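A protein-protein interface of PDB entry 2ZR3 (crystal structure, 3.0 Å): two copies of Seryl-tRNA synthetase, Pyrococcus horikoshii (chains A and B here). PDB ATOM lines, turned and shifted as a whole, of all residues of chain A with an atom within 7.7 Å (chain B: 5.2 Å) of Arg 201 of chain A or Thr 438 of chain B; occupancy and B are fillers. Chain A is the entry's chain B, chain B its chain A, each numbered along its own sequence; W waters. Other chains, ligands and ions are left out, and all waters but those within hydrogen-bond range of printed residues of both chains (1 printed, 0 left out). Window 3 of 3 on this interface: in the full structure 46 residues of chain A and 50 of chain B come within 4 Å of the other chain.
The guanidinium group (NH2) of Arg 201 of chain A lies within hydrogen-bond range of the backbone carbonyl oxygen (O) of Tyr 437 of chain B (2.6 Å).
O of Leu 434 of chain B sits at hydrogen-bond distance from OG1 of Thr 438 of chain B, at 2.9 Å. OG1 of Thr 438 of chain B is in hydrogen-bond range of O of Phe 440 of chain B. The guanidinium group (NE) of Arg 201 of chain A lies within salt-bridge range of the side-chain carboxylate (OD1) of Asp 205 of chain A (2.8 Å).
Ile 194 of chain B touches Arg 201 of chain A. O of Thr 438 of chain B touches NH1 of Arg 201 of chain A (3.8 Å). Leu 197 of chain B touches Leu 204 of chain A.
Of chain B, only Ile 194 (3.7 Å), Tyr 437 (2.6 Å) and Thr 438 (3.8 Å) come within 4 Å of Arg 201 of chain A. Of chain A, only Arg 201 (3.8 Å) comes within 4 Å of Thr 438 of chain B. Of the printed residues of chain A, Leu 197 of chain B touches Leu 204 (3.5 Å). Of the printed residues of chain A, Ile 194 of chain B touches Arg 201. Printed residues of chain A within 4 Å of Tyr 437 of chain B: Arg 201 (2.6 Å). Trp 435 of chain B touches none of the printed residues of chain A. The nearest residue of chain B that does not touch Arg 201 of chain A is Leu 197 of chain B (4.2 Å). The nearest residue of chain A that does not touch Thr 438 of chain B is Asp 205 of chain A (6.2 Å). The nearest printed residue of chain B that does not touch Leu 204 of chain A is Ile 194 of chain B (5.0 Å).
Printed residues of chain A that touch a printed residue of chain B: Arg 201 and Leu 204. Hydrophobic or aromatic side chains of chain A within 4 Å of the printed part of chain B: Leu 204. Among the printed residues, no Asp or Glu carboxylate lies within 4 Å of a Lys or Arg side-chain nitrogen of the other chain.
Positions printed for both chains: 194, 195, 197, 198, 434 and 437. Of the 4 pairs that touch across the chains among the printed residues, none has its exchanged pair printed and touching as well.
Water W1 bridges the guanidinium group (NH1) of Arg 201 of chain A (3.2 Å) and the backbone carbonyl oxygen (O) of Thr 438 of chain B (3.2 Å).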
ATOM      1  N   ILE A 194      -2.514   0.001 -32.885  1.00  0.00           N
ATOM      2  CA  ILE A 194      -1.284  -0.145 -32.115  1.00  0.00           C
ATOM      3  C   ILE A 194      -0.141   0.631 -32.772  1.00  0.00           C
ATOM      4  O   ILE A 194       0.665   1.254 -32.086  1.00  0.00           O
ATOM      5  CB  ILE A 194      -0.861  -1.629 -31.965  1.00  0.00           C
ATOM      6  CG1 ILE A 194      -1.967  -2.444 -31.295  1.00  0.00           C
ATOM      7  CG2 ILE A 194       0.358  -1.720 -31.101  1.00  0.00           C
ATOM      8  CD1 ILE A 194      -2.405  -1.886 -29.967  1.00  0.00           C
ATOM      9  N   LEU A 195      -0.070   0.591 -34.100  1.00  0.00           N
ATOM     10  CA  LEU A 195       0.976   1.319 -34.818  1.00  0.00           C
ATOM     11  C   LEU A 195       0.852   2.821 -34.551  1.00  0.00           C
ATOM     12  O   LEU A 195       1.849   3.517 -34.377  1.00  0.00           O
ATOM     13  CB  LEU A 195       0.889   1.053 -36.329  1.00  0.00           C
ATOM     14  CG  LEU A 195       1.866   1.870 -37.197  1.00  0.00           C
ATOM     15  CD1 LEU A 195       3.309   1.512 -36.870  1.00  0.00           C
ATOM     16  CD2 LEU A 195       1.609   1.602 -38.652  1.00  0.00           C
ATOM     17  N   ASP A 196      -0.378   3.316 -34.520  1.00  0.00           N
ATOM     18  CA  ASP A 196      -0.611   4.725 -34.258  1.00  0.00           C
ATOM     19  C   ASP A 196      -0.049   5.091 -32.879  1.00  0.00           C
ATOM     20  O   ASP A 196       0.678   6.070 -32.743  1.00  0.00           O
ATOM     21  CB  ASP A 196      -2.111   5.020 -34.309  1.00  0.00           C
ATOM     22  CG  ASP A 196      -2.420   6.493 -34.152  1.00  0.00           C
ATOM     23  OD1 ASP A 196      -1.926   7.107 -33.188  1.00  0.00           O
ATOM     24  OD2 ASP A 196      -3.170   7.042 -34.983  1.00  0.00           O
ATOM     25  N   LEU A 197      -0.368   4.304 -31.856  1.00  0.00           N
ATOM     26  CA  LEU A 197       0.124   4.608 -30.516  1.00  0.00           C
ATOM     27  C   LEU A 197       1.629   4.393 -30.387  1.00  0.00           C
ATOM     28  O   LEU A 197       2.307   5.088 -29.622  1.00  0.00           O
ATOM     29  CB  LEU A 197      -0.616   3.768 -29.476  1.00  0.00           C
ATOM     30  CG  LEU A 197      -2.124   4.022 -29.355  1.00  0.00           C
ATOM     31  CD1 LEU A 197      -2.643   3.246 -28.167  1.00  0.00           C
ATOM     32  CD2 LEU A 197      -2.428   5.511 -29.166  1.00  0.00           C
ATOM     33  N   ALA A 198       2.152   3.438 -31.145  1.00  0.00           N
ATOM     34  CA  ALA A 198       3.576   3.141 -31.118  1.00  0.00           C
ATOM     35  C   ALA A 198       4.376   4.305 -31.700  1.00  0.00           C
ATOM     36  O   ALA A 198       5.495   4.578 -31.272  1.00  0.00           O
ATOM     37  CB  ALA A 198       3.848   1.863 -31.894  1.00  0.00           C
ATOM     38  N   LEU A 199       3.813   4.999 -32.682  1.00  0.00           N
ATOM     39  CA  LEU A 199       4.521   6.134 -33.261  1.00  0.00           C
ATOM     40  C   LEU A 199       4.585   7.280 -32.257  1.00  0.00           C
ATOM     41  O   LEU A 199       5.604   7.962 -32.144  1.00  0.00           O
ATOM     42  CB  LEU A 199       3.834   6.603 -34.543  1.00  0.00           C
ATOM     43  CG  LEU A 199       4.027   5.694 -35.759  1.00  0.00           C
ATOM     44  CD1 LEU A 199       3.221   6.224 -36.930  1.00  0.00           C
ATOM     45  CD2 LEU A 199       5.500   5.627 -36.116  1.00  0.00           C
ATOM     46  N   ILE A 200       3.495   7.490 -31.527  1.00  0.00           N
ATOM     47  CA  ILE A 200       3.453   8.554 -30.545  1.00  0.00           C
ATOM     48  C   ILE A 200       4.507   8.298 -29.499  1.00  0.00           C
ATOM     49  O   ILE A 200       5.323   9.163 -29.193  1.00  0.00           O
ATOM     50  CB  ILE A 200       2.091   8.619 -29.840  1.00  0.00           C
ATOM     51  CG1 ILE A 200       1.023   9.019 -30.843  1.00  0.00           C
ATOM     52  CG2 ILE A 200       2.123   9.639 -28.706  1.00  0.00           C
ATOM     53  CD1 ILE A 200      -0.366   8.816 -30.337  1.00  0.00           C
ATOM     54  N   ARG A 201       4.484   7.096 -28.948  1.00  0.00           N
ATOM     55  CA  ARG A 201       5.425   6.747 -27.904  1.00  0.00           C
ATOM     56  C   ARG A 201       6.869   6.819 -28.397  1.00  0.00           C
ATOM     57  O   ARG A 201       7.741   7.404 -27.749  1.00  0.00           O
ATOM     58  CB  ARG A 201       5.089   5.362 -27.349  1.00  0.00           C
ATOM     59  CG  ARG A 201       5.895   4.976 -26.132  1.00  0.00           C
ATOM     60  CD  ARG A 201       5.860   6.038 -25.041  1.00  0.00           C
ATOM     61  NE  ARG A 201       7.019   5.881 -24.167  1.00  0.00           N
ATOM     62  CZ  ARG A 201       7.121   4.947 -23.227  1.00  0.00           C
ATOM     63  NH1 ARG A 201       8.223   4.864 -22.487  1.00  0.00           N
ATOM     64  NH2 ARG A 201       6.101   4.122 -23.008  1.00  0.00           N
ATOM     65  N   PHE A 202       7.119   6.250 -29.562  1.00  0.00           N
ATOM     66  CA  PHE A 202       8.456   6.276 -30.124  1.00  0.00           C
ATOM     67  C   PHE A 202       9.027   7.694 -30.267  1.00  0.00           C
ATOM     68  O   PHE A 202      10.211   7.904 -30.037  1.00  0.00           O
ATOM     69  CB  PHE A 202       8.454   5.575 -31.487  1.00  0.00           C
ATOM     70  CG  PHE A 202       9.638   5.918 -32.347  1.00  0.00           C
ATOM     71  CD1 PHE A 202      10.931   5.662 -31.910  1.00  0.00           C
ATOM     72  CD2 PHE A 202       9.458   6.506 -33.596  1.00  0.00           C
ATOM     73  CE1 PHE A 202      12.028   5.989 -32.707  1.00  0.00           C
ATOM     74  CE2 PHE A 202      10.553   6.835 -34.401  1.00  0.00           C
ATOM     75  CZ  PHE A 202      11.839   6.577 -33.955  1.00  0.00           C
ATOM     76  N   ALA A 203       8.190   8.659 -30.643  1.00  0.00           N
ATOM     77  CA  ALA A 203       8.632  10.041 -30.842  1.00  0.00           C
ATOM     78  C   ALA A 203       8.839  10.737 -29.506  1.00  0.00           C
ATOM     79  O   ALA A 203       9.757  11.544 -29.325  1.00  0.00           O
ATOM     80  CB  ALA A 203       7.611  10.799 -31.682  1.00  0.00           C
ATOM     81  N   LEU A 204       7.965  10.413 -28.575  1.00  0.00           N
ATOM     82  CA  LEU A 204       8.028  10.960 -27.240  1.00  0.00           C
ATOM     83  C   LEU A 204       9.310  10.453 -26.567  1.00  0.00           C
ATOM     84  O   LEU A 204      10.013  11.205 -25.880  1.00  0.00           O
ATOM     85  CB  LEU A 204       6.813  10.474 -26.473  1.00  0.00           C
ATOM     86  CG  LEU A 204       5.968  11.465 -25.704  1.00  0.00           C
ATOM     87  CD1 LEU A 204       6.057  12.847 -26.308  1.00  0.00           C
ATOM     88  CD2 LEU A 204       4.547  10.923 -25.711  1.00  0.00           C
ATOM     89  N   ASP A 205       9.612   9.169 -26.766  1.00  0.00           N
ATOM     90  CA  ASP A 205      10.797   8.588 -26.146  1.00  0.00           C
ATOM     91  C   ASP A 205      12.055   9.262 -26.639  1.00  0.00           C
ATOM     92  O   ASP A 205      12.878   9.717 -25.849  1.00  0.00           O
ATOM     93  CB  ASP A 205      10.885   7.081 -26.411  1.00  0.00           C
ATOM     94  CG  ASP A 205      10.166   6.241 -25.346  1.00  0.00           C
ATOM     95  OD1 ASP A 205       9.617   6.819 -24.366  1.00  0.00           O
ATOM     96  OD2 ASP A 205      10.162   4.992 -25.496  1.00  0.00           O
ATOM     97  N   ARG A 206      12.200   9.356 -27.951  1.00  0.00           N
ATOM     98  CA  ARG A 206      13.397   9.961 -28.497  1.00  0.00           C
ATOM     99  C   ARG A 206      13.518  11.455 -28.194  1.00  0.00           C
ATOM    100  O   ARG A 206      14.622  11.987 -28.172  1.00  0.00           O
ATOM    101  CB  ARG A 206      13.470   9.709 -30.004  1.00  0.00           C
ATOM    102  CG  ARG A 206      14.836   9.181 -30.471  1.00  0.00           C
ATOM    103  CD  ARG A 206      15.172   7.855 -29.804  1.00  0.00           C
ATOM    104  NE  ARG A 206      15.318   6.752 -30.756  1.00  0.00           N
ATOM    105  CZ  ARG A 206      15.071   5.470 -30.465  1.00  0.00           C
ATOM    106  NH1 ARG A 206      14.660   5.116 -29.249  1.00  0.00           N
ATOM    107  NH2 ARG A 206      15.235   4.535 -31.393  1.00  0.00           N
ATOM    108  N   LEU A 207      12.407  12.139 -27.947  1.00  0.00           N
ATOM    109  CA  LEU A 207      12.508  13.568 -27.665  1.00  0.00           C
ATOM    110  C   LEU A 207      12.841  13.820 -26.203  1.00  0.00           C
ATOM    111  O   LEU A 207      13.522  14.803 -25.864  1.00  0.00           O
ATOM    112  CB  LEU A 207      11.225  14.299 -28.074  1.00  0.00           C
ATOM    113  CG  LEU A 207      11.293  14.894 -29.489  1.00  0.00           C
ATOM    114  CD1 LEU A 207      12.330  15.977 -29.558  1.00  0.00           C
ATOM    115  CD2 LEU A 207      11.625  13.810 -30.488  1.00  0.00           C
ATOM    116  N   ILE A 208      12.352  12.933 -25.340  1.00  0.00           N
ATOM    117  CA  ILE A 208      12.654  13.022 -23.918  1.00  0.00           C
ATOM    118  C   ILE A 208      14.167  12.719 -23.759  1.00  0.00           C
ATOM    119  O   ILE A 208      14.873  13.374 -22.973  1.00  0.00           O
ATOM    120  CB  ILE A 208      11.805  12.012 -23.114  1.00  0.00           C
ATOM    121  CG1 ILE A 208      10.355  12.484 -23.074  1.00  0.00           C
ATOM    122  CG2 ILE A 208      12.343  11.868 -21.709  1.00  0.00           C
ATOM    123  CD1 ILE A 208       9.408  11.529 -22.383  1.00  0.00           C
ATOM    124  N   VAL A 278       1.816  16.101 -26.972  1.00  0.00           N
ATOM    125  CA  VAL A 278       1.099  15.047 -27.691  1.00  0.00           C
ATOM    126  C   VAL A 278      -0.344  15.460 -27.604  1.00  0.00           C
ATOM    127  O   VAL A 278      -0.774  15.956 -26.567  1.00  0.00           O
ATOM    128  CB  VAL A 278       1.158  13.673 -27.005  1.00  0.00           C
ATOM    129  CG1 VAL A 278       0.676  12.615 -27.979  1.00  0.00           C
ATOM    130  CG2 VAL A 278       2.544  13.378 -26.507  1.00  0.00           C
ATOM    131  N   VAL A 305       2.785  14.478 -32.383  1.00  0.00           N
ATOM    132  CA  VAL A 305       3.733  14.800 -31.313  1.00  0.00           C
ATOM    133  C   VAL A 305       4.511  16.031 -31.791  1.00  0.00           C
ATOM    134  O   VAL A 305       5.198  15.981 -32.811  1.00  0.00           O
ATOM    135  CB  VAL A 305       4.704  13.637 -31.060  1.00  0.00           C
ATOM    136  CG1 VAL A 305       5.795  14.084 -30.102  1.00  0.00           C
ATOM    137  CG2 VAL A 305       3.930  12.426 -30.501  1.00  0.00           C
ATOM    138  N   ILE A 408       6.289  13.673 -35.171  1.00  0.00           N
ATOM    139  CA  ILE A 408       5.577  12.709 -35.992  1.00  0.00           C
ATOM    140  C   ILE A 408       4.084  12.981 -35.898  1.00  0.00           C
ATOM    141  O   ILE A 408       3.549  13.161 -34.808  1.00  0.00           O
ATOM    142  CB  ILE A 408       5.805  11.249 -35.536  1.00  0.00           C
ATOM    143  CG1 ILE A 408       7.256  10.834 -35.722  1.00  0.00           C
ATOM    144  CG2 ILE A 408       4.954  10.307 -36.364  1.00  0.00           C
ATOM    145  CD1 ILE A 408       7.504   9.389 -35.342  1.00  0.00           C
ATOM    146  N   THR A 410       1.089  10.998 -36.573  1.00  0.00           N
ATOM    147  CA  THR A 410       0.723   9.609 -36.866  1.00  0.00           C
ATOM    148  C   THR A 410       0.057   9.299 -38.188  1.00  0.00           C
ATOM    149  O   THR A 410       0.478   8.381 -38.894  1.00  0.00           O
ATOM    150  CB  THR A 410      -0.159   9.005 -35.768  1.00  0.00           C
ATOM    151  OG1 THR A 410      -1.419   9.692 -35.722  1.00  0.00           O
ATOM    152  CG2 THR A 410       0.541   9.108 -34.437  1.00  0.00           C
ATOM    153  N   LEU A 434      10.540   0.160 -34.556  1.00  0.00           N
ATOM    154  CA  LEU A 434       9.217   0.188 -33.960  1.00  0.00           C
ATOM    155  C   LEU A 434       8.791  -1.126 -33.348  1.00  0.00           C
ATOM    156  O   LEU A 434       7.674  -1.222 -32.839  1.00  0.00           O
ATOM    157  CB  LEU A 434       8.162   0.580 -34.987  1.00  0.00           C
ATOM    158  CG  LEU A 434       8.055   2.012 -35.493  1.00  0.00           C
ATOM    159  CD1 LEU A 434       6.839   2.128 -36.418  1.00  0.00           C
ATOM    160  CD2 LEU A 434       7.925   2.951 -34.319  1.00  0.00           C
ATOM    161  N   TYR A 437       7.830  -1.422 -29.617  1.00  0.00           N
ATOM    162  CA  TYR A 437       6.538  -0.844 -29.265  1.00  0.00           C
ATOM    163  C   TYR A 437       5.337  -1.615 -29.798  1.00  0.00           C
ATOM    164  O   TYR A 437       4.306  -1.658 -29.136  1.00  0.00           O
ATOM    165  CB  TYR A 437       6.424   0.618 -29.726  1.00  0.00           C
ATOM    166  CG  TYR A 437       7.553   1.528 -29.283  1.00  0.00           C
ATOM    167  CD1 TYR A 437       8.697   1.685 -30.067  1.00  0.00           C
ATOM    168  CD2 TYR A 437       7.487   2.227 -28.077  1.00  0.00           C
ATOM    169  CE1 TYR A 437       9.750   2.518 -29.661  1.00  0.00           C
ATOM    170  CE2 TYR A 437       8.546   3.064 -27.660  1.00  0.00           C
ATOM    171  CZ  TYR A 437       9.670   3.199 -28.459  1.00  0.00           C
ATOM    172  OH  TYR A 437      10.714   3.999 -28.055  1.00  0.00           O
ATOM    173  N   ILE B 194       3.781   9.711 -19.584  1.00  0.00           N
ATOM    174  CA  ILE B 194       4.107   8.340 -19.946  1.00  0.00           C
ATOM    175  C   ILE B 194       3.134   7.407 -19.248  1.00  0.00           C
ATOM    176  O   ILE B 194       2.584   6.497 -19.858  1.00  0.00           O
ATOM    177  CB  ILE B 194       5.493   7.924 -19.477  1.00  0.00           C
ATOM    178  CG1 ILE B 194       6.568   8.745 -20.189  1.00  0.00           C
ATOM    179  CG2 ILE B 194       5.679   6.437 -19.731  1.00  0.00           C
ATOM    180  CD1 ILE B 194       6.559   8.591 -21.686  1.00  0.00           C
ATOM    181  N   LEU B 195       2.940   7.625 -17.952  1.00  0.00           N
ATOM    182  CA  LEU B 195       2.033   6.787 -17.188  1.00  0.00           C
ATOM    183  C   LEU B 195       0.686   6.713 -17.908  1.00  0.00           C
ATOM    184  O   LEU B 195       0.131   5.622 -18.081  1.00  0.00           O
ATOM    185  CB  LEU B 195       1.875   7.329 -15.755  1.00  0.00           C
ATOM    186  CG  LEU B 195       0.905   6.559 -14.840  1.00  0.00           C
ATOM    187  CD1 LEU B 195       1.333   5.122 -14.712  1.00  0.00           C
ATOM    188  CD2 LEU B 195       0.863   7.193 -13.483  1.00  0.00           C
ATOM    189  N   LEU B 197      -0.138   7.253 -21.215  1.00  0.00           N
ATOM    190  CA  LEU B 197      -0.062   6.399 -22.396  1.00  0.00           C
ATOM    191  C   LEU B 197       0.096   4.961 -21.967  1.00  0.00           C
ATOM    192  O   LEU B 197      -0.457   4.050 -22.588  1.00  0.00           O
ATOM    193  CB  LEU B 197       1.129   6.767 -23.273  1.00  0.00           C
ATOM    194  CG  LEU B 197       1.216   8.217 -23.745  1.00  0.00           C
ATOM    195  CD1 LEU B 197       2.376   8.320 -24.724  1.00  0.00           C
ATOM    196  CD2 LEU B 197      -0.099   8.681 -24.396  1.00  0.00           C
ATOM    197  N   ALA B 198       0.867   4.779 -20.900  1.00  0.00           N
ATOM    198  CA  ALA B 198       1.152   3.468 -20.332  1.00  0.00           C
ATOM    199  C   ALA B 198      -0.137   2.711 -20.032  1.00  0.00           C
ATOM    200  O   ALA B 198      -0.309   1.556 -20.441  1.00  0.00           O
ATOM    201  CB  ALA B 198       1.968   3.635 -19.064  1.00  0.00           C
ATOM    202  N   ILE B 430       5.345   2.512  -9.137  1.00  0.00           N
ATOM    203  CA  ILE B 430       4.499   2.053 -10.213  1.00  0.00           C
ATOM    204  C   ILE B 430       4.308   0.552 -10.086  1.00  0.00           C
ATOM    205  O   ILE B 430       5.245  -0.168  -9.771  1.00  0.00           O
ATOM    206  CB  ILE B 430       5.109   2.395 -11.595  1.00  0.00           C
ATOM    207  CG1 ILE B 430       4.781   3.842 -11.970  1.00  0.00           C
ATOM    208  CG2 ILE B 430       4.544   1.479 -12.659  1.00  0.00           C
ATOM    209  CD1 ILE B 430       5.364   4.867 -11.055  1.00  0.00           C
ATOM    210  N   LEU B 434       2.903  -2.411 -15.054  1.00  0.00           N
ATOM    211  CA  LEU B 434       3.176  -1.272 -15.938  1.00  0.00           C
ATOM    212  C   LEU B 434       4.640  -0.966 -16.238  1.00  0.00           C
ATOM    213  O   LEU B 434       4.939  -0.064 -17.018  1.00  0.00           O
ATOM    214  CB  LEU B 434       2.555  -0.005 -15.361  1.00  0.00           C
ATOM    215  CG  LEU B 434       1.043   0.006 -15.261  1.00  0.00           C
ATOM    216  CD1 LEU B 434       0.599   1.290 -14.593  1.00  0.00           C
ATOM    217  CD2 LEU B 434       0.453  -0.128 -16.646  1.00  0.00           C
ATOM    218  N   TRP B 435       5.558  -1.693 -15.622  1.00  0.00           N
ATOM    219  CA  TRP B 435       6.966  -1.430 -15.874  1.00  0.00           C
ATOM    220  C   TRP B 435       7.368  -1.545 -17.350  1.00  0.00           C
ATOM    221  O   TRP B 435       8.124  -0.709 -17.848  1.00  0.00           O
ATOM    222  CB  TRP B 435       7.836  -2.336 -14.998  1.00  0.00           C
ATOM    223  CG  TRP B 435       7.736  -1.993 -13.538  1.00  0.00           C
ATOM    224  CD1 TRP B 435       7.081  -0.926 -12.990  1.00  0.00           C
ATOM    225  CD2 TRP B 435       8.313  -2.710 -12.442  1.00  0.00           C
ATOM    226  NE1 TRP B 435       7.213  -0.934 -11.621  1.00  0.00           N
ATOM    227  CE2 TRP B 435       7.962  -2.020 -11.260  1.00  0.00           C
ATOM    228  CE3 TRP B 435       9.087  -3.869 -12.343  1.00  0.00           C
ATOM    229  CZ2 TRP B 435       8.363  -2.449 -10.002  1.00  0.00           C
ATOM    230  CZ3 TRP B 435       9.485  -4.292 -11.095  1.00  0.00           C
ATOM    231  CH2 TRP B 435       9.121  -3.585  -9.938  1.00  0.00           C
ATOM    232  N   LYS B 436       6.859  -2.551 -18.060  1.00  0.00           N
ATOM    233  CA  LYS B 436       7.220  -2.703 -19.464  1.00  0.00           C
ATOM    234  C   LYS B 436       6.741  -1.535 -20.313  1.00  0.00           C
ATOM    235  O   LYS B 436       7.293  -1.264 -21.392  1.00  0.00           O
ATOM    236  CB  LYS B 436       6.690  -4.026 -20.036  1.00  0.00           C
ATOM    237  CG  LYS B 436       5.236  -4.349 -19.762  1.00  0.00           C
ATOM    238  CD  LYS B 436       4.878  -5.707 -20.382  1.00  0.00           C
ATOM    239  CE  LYS B 436       3.450  -6.165 -20.053  1.00  0.00           C
ATOM    240  NZ  LYS B 436       3.234  -6.521 -18.612  1.00  0.00           N
ATOM    241  N   TYR B 437       5.730  -0.825 -19.821  1.00  0.00           N
ATOM    242  CA  TYR B 437       5.203   0.306 -20.560  1.00  0.00           C
ATOM    243  C   TYR B 437       5.808   1.640 -20.146  1.00  0.00           C
ATOM    244  O   TYR B 437       6.048   2.496 -20.992  1.00  0.00           O
ATOM    245  CB  TYR B 437       3.681   0.384 -20.418  1.00  0.00           C
ATOM    246  CG  TYR B 437       2.937  -0.878 -20.804  1.00  0.00           C
ATOM    247  CD1 TYR B 437       2.579  -1.805 -19.844  1.00  0.00           C
ATOM    248  CD2 TYR B 437       2.555  -1.122 -22.126  1.00  0.00           C
ATOM    249  CE1 TYR B 437       1.859  -2.937 -20.168  1.00  0.00           C
ATOM    250  CE2 TYR B 437       1.825  -2.264 -22.464  1.00  0.00           C
ATOM    251  CZ  TYR B 437       1.478  -3.167 -21.469  1.00  0.00           C
ATOM    252  OH  TYR B 437       0.729  -4.294 -21.740  1.00  0.00           O
ATOM    253  N   THR B 438       6.069   1.812 -18.856  1.00  0.00           N
ATOM    254  CA  THR B 438       6.598   3.073 -18.346  1.00  0.00           C
ATOM    255  C   THR B 438       8.090   3.255 -18.430  1.00  0.00           C
ATOM    256  O   THR B 438       8.579   4.348 -18.736  1.00  0.00           O
ATOM    257  CB  THR B 438       6.256   3.252 -16.883  1.00  0.00           C
ATOM    258  OG1 THR B 438       6.658   2.070 -16.186  1.00  0.00           O
ATOM    259  CG2 THR B 438       4.762   3.489 -16.684  1.00  0.00           C
ATOM    260  N   GLY B 439       8.811   2.186 -18.130  1.00  0.00           N
ATOM    261  CA  GLY B 439      10.257   2.262 -18.121  1.00  0.00           C
ATOM    262  C   GLY B 439      10.667   2.398 -16.665  1.00  0.00           C
ATOM    263  O   GLY B 439      11.181   1.453 -16.081  1.00  0.00           O
ATOM    264  N   PHE B 440      10.414   3.562 -16.075  1.00  0.00           N
ATOM    265  CA  PHE B 440      10.746   3.830 -14.681  1.00  0.00           C
ATOM    266  C   PHE B 440       9.930   2.918 -13.768  1.00  0.00           C
ATOM    267  O   PHE B 440       8.913   2.370 -14.206  1.00  0.00           O
ATOM    268  CB  PHE B 440      10.444   5.289 -14.374  1.00  0.00           C
ATOM    269  CG  PHE B 440       9.096   5.740 -14.858  1.00  0.00           C
ATOM    270  CD1 PHE B 440       7.957   5.506 -14.107  1.00  0.00           C
ATOM    271  CD2 PHE B 440       8.968   6.422 -16.062  1.00  0.00           C
ATOM    272  CE1 PHE B 440       6.717   5.954 -14.556  1.00  0.00           C
ATOM    273  CE2 PHE B 440       7.733   6.868 -16.509  1.00  0.00           C
ATOM    274  CZ  PHE B 440       6.612   6.637 -15.760  1.00  0.00           C
HETATM  275  O   HOH W   1      10.279   6.350 -20.591  1.00  0.00           O
